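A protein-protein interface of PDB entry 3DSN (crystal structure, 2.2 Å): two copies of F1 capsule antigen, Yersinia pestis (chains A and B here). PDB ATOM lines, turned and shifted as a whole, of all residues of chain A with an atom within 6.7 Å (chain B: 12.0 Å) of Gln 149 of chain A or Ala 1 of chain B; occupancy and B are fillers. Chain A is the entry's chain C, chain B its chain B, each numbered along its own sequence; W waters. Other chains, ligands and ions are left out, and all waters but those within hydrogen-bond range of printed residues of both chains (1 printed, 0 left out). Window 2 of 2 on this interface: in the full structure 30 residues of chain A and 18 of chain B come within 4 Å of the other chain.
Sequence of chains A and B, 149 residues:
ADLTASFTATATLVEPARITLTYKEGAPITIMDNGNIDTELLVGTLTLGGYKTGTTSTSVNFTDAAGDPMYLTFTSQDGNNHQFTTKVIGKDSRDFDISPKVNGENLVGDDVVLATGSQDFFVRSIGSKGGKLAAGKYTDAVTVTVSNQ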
ATOM      1  N   ILE A  19     -31.148 -24.501  15.159  1.00  0.00           N
ATOM      2  CA  ILE A  19     -30.840 -24.769  13.755  1.00  0.00           C
ATOM      3  C   ILE A  19     -31.499 -26.093  13.336  1.00  0.00           C
ATOM      4  O   ILE A  19     -31.406 -27.098  14.049  1.00  0.00           O
ATOM      5  CB  ILE A  19     -29.290 -24.850  13.543  1.00  0.00           C
ATOM      6  CG1 ILE A  19     -28.602 -23.519  13.899  1.00  0.00           C
ATOM      7  CG2 ILE A  19     -28.904 -25.314  12.124  1.00  0.00           C
ATOM      8  CD1 ILE A  19     -29.072 -22.299  13.123  1.00  0.00           C
ATOM      9  N   GLY A  50     -33.691 -21.871  10.800  1.00  0.00           N
ATOM     10  CA  GLY A  50     -33.614 -21.476  12.202  1.00  0.00           C
ATOM     11  C   GLY A  50     -32.409 -20.620  12.571  1.00  0.00           C
ATOM     12  O   GLY A  50     -32.106 -20.447  13.769  1.00  0.00           O
ATOM     13  N   TYR A  51     -31.711 -20.093  11.564  1.00  0.00           N
ATOM     14  CA  TYR A  51     -30.553 -19.206  11.785  1.00  0.00           C
ATOM     15  C   TYR A  51     -30.962 -17.731  11.918  1.00  0.00           C
ATOM     16  O   TYR A  51     -31.989 -17.313  11.353  1.00  0.00           O
ATOM     17  CB  TYR A  51     -29.509 -19.368  10.662  1.00  0.00           C
ATOM     18  CG  TYR A  51     -30.090 -19.359   9.254  1.00  0.00           C
ATOM     19  CD1 TYR A  51     -30.466 -18.153   8.629  1.00  0.00           C
ATOM     20  CD2 TYR A  51     -30.263 -20.558   8.547  1.00  0.00           C
ATOM     21  CE1 TYR A  51     -31.000 -18.147   7.348  1.00  0.00           C
ATOM     22  CE2 TYR A  51     -30.802 -20.571   7.253  1.00  0.00           C
ATOM     23  CZ  TYR A  51     -31.165 -19.367   6.665  1.00  0.00           C
ATOM     24  OH  TYR A  51     -31.680 -19.374   5.403  1.00  0.00           O
ATOM     25  N   LYS A  52     -30.158 -16.963  12.658  1.00  0.00           N
ATOM     26  CA  LYS A  52     -30.360 -15.514  12.851  1.00  0.00           C
ATOM     27  C   LYS A  52     -30.404 -14.745  11.519  1.00  0.00           C
ATOM     28  O   LYS A  52     -29.750 -15.147  10.551  1.00  0.00           O
ATOM     29  CB  LYS A  52     -29.255 -14.958  13.790  1.00  0.00           C
ATOM     30  CG  LYS A  52     -28.973 -13.442  13.686  1.00  0.00           C
ATOM     31  CD  LYS A  52     -28.255 -12.792  14.907  1.00  0.00           C
ATOM     32  CE  LYS A  52     -26.767 -13.162  14.985  1.00  0.00           C
ATOM     33  NZ  LYS A  52     -25.894 -12.046  15.503  1.00  0.00           N
ATOM     34  N   THR A  53     -31.163 -13.644  11.465  1.00  0.00           N
ATOM     35  CA  THR A  53     -31.210 -12.797  10.265  1.00  0.00           C
ATOM     36  C   THR A  53     -29.830 -12.199  10.024  1.00  0.00           C
ATOM     37  O   THR A  53     -29.121 -11.862  10.974  1.00  0.00           O
ATOM     38  CB  THR A  53     -32.252 -11.637  10.384  1.00  0.00           C
ATOM     39  OG1 THR A  53     -33.165 -11.893  11.469  1.00  0.00           O
ATOM     40  CG2 THR A  53     -33.038 -11.441   9.052  1.00  0.00           C
ATOM     41  N   THR A  55     -27.348 -13.967   8.762  1.00  0.00           N
ATOM     42  CA  THR A  55     -26.391 -15.079   8.653  1.00  0.00           C
ATOM     43  C   THR A  55     -25.881 -15.191   7.206  1.00  0.00           C
ATOM     44  O   THR A  55     -26.646 -15.120   6.267  1.00  0.00           O
ATOM     45  CB  THR A  55     -26.988 -16.420   9.197  1.00  0.00           C
ATOM     46  OG1 THR A  55     -27.352 -16.243  10.569  1.00  0.00           O
ATOM     47  CG2 THR A  55     -25.964 -17.577   9.112  1.00  0.00           C
ATOM     48  N   THR A  56     -24.572 -15.281   7.043  1.00  0.00           N
ATOM     49  CA  THR A  56     -23.964 -15.364   5.715  1.00  0.00           C
ATOM     50  C   THR A  56     -23.523 -16.801   5.405  1.00  0.00           C
ATOM     51  O   THR A  56     -23.364 -17.631   6.300  1.00  0.00           O
ATOM     52  CB  THR A  56     -22.740 -14.407   5.553  1.00  0.00           C
ATOM     53  OG1 THR A  56     -21.711 -14.786   6.475  1.00  0.00           O
ATOM     54  CG2 THR A  56     -23.114 -12.947   5.786  1.00  0.00           C
ATOM     55  N   SER A  59     -20.718 -18.579   7.444  1.00  0.00           N
ATOM     56  CA  SER A  59     -21.033 -18.991   8.801  1.00  0.00           C
ATOM     57  C   SER A  59     -21.606 -20.410   8.817  1.00  0.00           C
ATOM     58  O   SER A  59     -21.923 -20.935   9.862  1.00  0.00           O
ATOM     59  CB  SER A  59     -22.058 -18.028   9.414  1.00  0.00           C
ATOM     60  OG  SER A  59     -21.498 -16.761   9.669  1.00  0.00           O
ATOM     61  N   VAL A 146     -23.496 -23.727  12.315  1.00  0.00           N
ATOM     62  CA  VAL A 146     -23.779 -22.354  11.926  1.00  0.00           C
ATOM     63  C   VAL A 146     -23.194 -21.417  12.983  1.00  0.00           C
ATOM     64  O   VAL A 146     -23.622 -21.419  14.144  1.00  0.00           O
ATOM     65  CB  VAL A 146     -25.293 -22.108  11.714  1.00  0.00           C
ATOM     66  CG1 VAL A 146     -25.546 -20.672  11.307  1.00  0.00           C
ATOM     67  CG2 VAL A 146     -25.859 -23.087  10.660  1.00  0.00           C
ATOM     68  N   SER A 147     -22.217 -20.625  12.550  1.00  0.00           N
ATOM     69  CA  SER A 147     -21.497 -19.699  13.399  1.00  0.00           C
ATOM     70  C   SER A 147     -22.219 -18.397  13.554  1.00  0.00           C
ATOM     71  O   SER A 147     -23.205 -18.115  12.865  1.00  0.00           O
ATOM     72  CB  SER A 147     -20.149 -19.371  12.775  1.00  0.00           C
ATOM     73  OG  SER A 147     -19.392 -20.541  12.605  1.00  0.00           O
ATOM     74  N   ASN A 148     -21.664 -17.594  14.454  1.00  0.00           N
ATOM     75  CA  ASN A 148     -22.073 -16.213  14.679  1.00  0.00           C
ATOM     76  C   ASN A 148     -23.548 -16.030  14.960  1.00  0.00           C
ATOM     77  O   ASN A 148     -24.148 -15.040  14.540  1.00  0.00           O
ATOM     78  CB  ASN A 148     -21.601 -15.330  13.526  1.00  0.00           C
ATOM     79  CG  ASN A 148     -20.118 -15.466  13.281  1.00  0.00           C
ATOM     80  OD1 ASN A 148     -19.299 -15.115  14.135  1.00  0.00           O
ATOM     81  ND2 ASN A 148     -19.758 -15.988  12.110  1.00  0.00           N
ATOM     82  N   GLN A 149     -24.111 -16.991  15.685  1.00  0.00           N
ATOM     83  CA  GLN A 149     -25.506 -16.960  16.128  1.00  0.00           C
ATOM     84  C   GLN A 149     -25.645 -16.295  17.486  1.00  0.00           C
ATOM     85  O   GLN A 149     -24.801 -16.448  18.385  1.00  0.00           O
ATOM     86  CB  GLN A 149     -26.110 -18.377  16.185  1.00  0.00           C
ATOM     87  CG  GLN A 149     -26.117 -19.088  14.844  1.00  0.00           C
ATOM     88  CD  GLN A 149     -26.806 -18.272  13.757  1.00  0.00           C
ATOM     89  OE1 GLN A 149     -28.025 -18.179  13.718  1.00  0.00           O
ATOM     90  NE2 GLN A 149     -26.018 -17.684  12.870  1.00  0.00           N
ATOM     91  OXT GLN A 149     -26.635 -15.600  17.703  1.00  0.00           O
ATOM     92  N   ALA B   1     -22.321 -17.398  18.790  1.00  0.00           N
ATOM     93  CA  ALA B   1     -22.380 -18.834  19.190  1.00  0.00           C
ATOM     94  C   ALA B   1     -22.537 -19.753  17.980  1.00  0.00           C
ATOM     95  O   ALA B   1     -23.118 -19.367  16.946  1.00  0.00           O
ATOM     96  CB  ALA B   1     -23.522 -19.064  20.171  1.00  0.00           C
ATOM     97  N   ASP B   2     -22.011 -20.966  18.129  1.00  0.00           N
ATOM     98  CA  ASP B   2     -22.152 -22.026  17.138  1.00  0.00           C
ATOM     99  C   ASP B   2     -23.324 -22.903  17.503  1.00  0.00           C
ATOM    100  O   ASP B   2     -23.410 -23.395  18.633  1.00  0.00           O
ATOM    101  CB  ASP B   2     -20.874 -22.874  17.072  1.00  0.00           C
ATOM    102  CG  ASP B   2     -19.717 -22.135  16.426  1.00  0.00           C
ATOM    103  OD1 ASP B   2     -18.677 -22.771  16.161  1.00  0.00           O
ATOM    104  OD2 ASP B   2     -19.835 -20.910  16.179  1.00  0.00           O
ATOM    105  N   LEU B   3     -24.243 -23.076  16.560  1.00  0.00           N
ATOM    106  CA  LEU B   3     -25.338 -24.035  16.724  1.00  0.00           C
ATOM    107  C   LEU B   3     -25.196 -25.109  15.651  1.00  0.00           C
ATOM    108  O   LEU B   3     -24.697 -24.835  14.556  1.00  0.00           O
ATOM    109  CB  LEU B   3     -26.699 -23.340  16.656  1.00  0.00           C
ATOM    110  CG  LEU B   3     -26.967 -22.131  17.567  1.00  0.00           C
ATOM    111  CD1 LEU B   3     -28.343 -21.565  17.290  1.00  0.00           C
ATOM    112  CD2 LEU B   3     -26.817 -22.490  19.047  1.00  0.00           C
ATOM    113  N   THR B   4     -25.591 -26.336  15.980  1.00  0.00           N
ATOM    114  CA  THR B   4     -25.394 -27.464  15.077  1.00  0.00           C
ATOM    115  C   THR B   4     -26.697 -28.199  14.817  1.00  0.00           C
ATOM    116  O   THR B   4     -27.650 -28.103  15.600  1.00  0.00           O
ATOM    117  CB  THR B   4     -24.368 -28.505  15.614  1.00  0.00           C
ATOM    118  OG1 THR B   4     -24.907 -29.139  16.775  1.00  0.00           O
ATOM    119  CG2 THR B   4     -23.012 -27.865  15.940  1.00  0.00           C
ATOM    120  N   ALA B   5     -26.713 -28.942  13.718  1.00  0.00           N
ATOM    121  CA  ALA B   5     -27.731 -29.936  13.451  1.00  0.00           C
ATOM    122  C   ALA B   5     -27.089 -31.006  12.562  1.00  0.00           C
ATOM    123  O   ALA B   5     -25.961 -30.864  12.115  1.00  0.00           O
ATOM    124  CB  ALA B   5     -28.955 -29.276  12.758  1.00  0.00           C
HETATM  125  O   HOH W   1     -19.920 -18.192  16.726  1.00  0.00           O
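The backbone NH of Asn 148 of chain A sits at hydrogen-bond distance from the backbone carbonyl oxygen of Ala 1 of chain B (3.4 Å).
The backbone NH (N) of Ala 1 of chain B lies within hydrogen-bond range of the chain-end carboxylate (O) of Gln 149 of chain A (2.7 Å).
O of Leu 3 of chain B is in hydrogen-bond range of N of Val 146 of chain A, 2.8 Å away.
The side-chain amide oxygen (OE1) of Gln 149 of chain A lies within hydrogen-bond range of the backbone NH (N) of Lys 52 of chain A, at 2.7 Å.
OG1 of Thr 55 of chain A sits at hydrogen-bond distance from NE2 of Gln 149 of chain A, 3.0 Å away.
The backbone carbonyl oxygen of Ser 59 of chain A is in hydrogen-bond range of the backbone NH of Ser 147 of chain A.
OG of Ser 59 of chain A sits at hydrogen-bond distance from ND2 of Asn 148 of chain A (3.1 Å).
O of Ser 147 of chain A is in hydrogen-bond range of NE2 of Gln 149 of chain A, 2.8 Å away.
Among the printed residues, pairs that only touch across the chains: Ile 19 of chain A with Leu 3 of chain B, Ile 19 of chain A with Ala 5 of chain B, Val 146 of chain A with Ala 1 of chain B, Val 146 of chain A with Asp 2 of chain B, Ser 147 of chain A with Ala 1 of chain B and Ser 147 of chain A with Asp 2 of chain B.
Gln 149 of chain A touches one residue of chain B.
No residue of chain B comes within 4 Å of Thr 55 of chain A.
No residue of chain B comes within 4 Å of Ser 59 of chain A.
Of the printed residues of chain B, Val 146 of chain A touches Ala 1, Asp 2 and Leu 3.
Asn 148 of chain A touches just one residue of chain B: Ala 1.
Printed residues of chain A within 4 Å of Leu 3 of chain B: Ile 19 and Val 146.
Of the printed residues of chain B, Ile 19 of chain A touches Leu 3 and Ala 5.
Printed residues of chain A within 4 Å of Asp 2 of chain B: Val 146 (3.4 Å) and Ser 147 (3.5 Å).
Printed residues of chain A within 4 Å of Ala 5 of chain B: Ile 19.
Thr 56 of chain A touches none of the printed residues of chain B.
Thr 4 of chain B touches none of the printed residues of chain A.
The nearest printed residue of chain B that does not touch Ile 19 of chain A is Thr 4 of chain B (4.2 Å).
Of the 5 printed residues of chain B, 4 touch a printed residue of chain A.
Printed residues of chain B that touch a printed residue of chain A: Ala 1, Asp 2, Leu 3 and Ala 5.
Along chain A the printed residues that touch a printed residue of chain B span positions 19 to 149.
Among the printed residues, 9 pairs touch across the chains.
Among the printed residues, no Asp or Glu carboxylate lies within 4 Å of a Lys or Arg side-chain nitrogen of the other chain.
No position is printed for both chains.
Water W1 lies within hydrogen-bond range of OD2 of Asp 2 of chain B (2.8 Å), N of Asn 148 of chain A (2.9 Å) and N of Ala 1 of chain B (3.3 Å).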
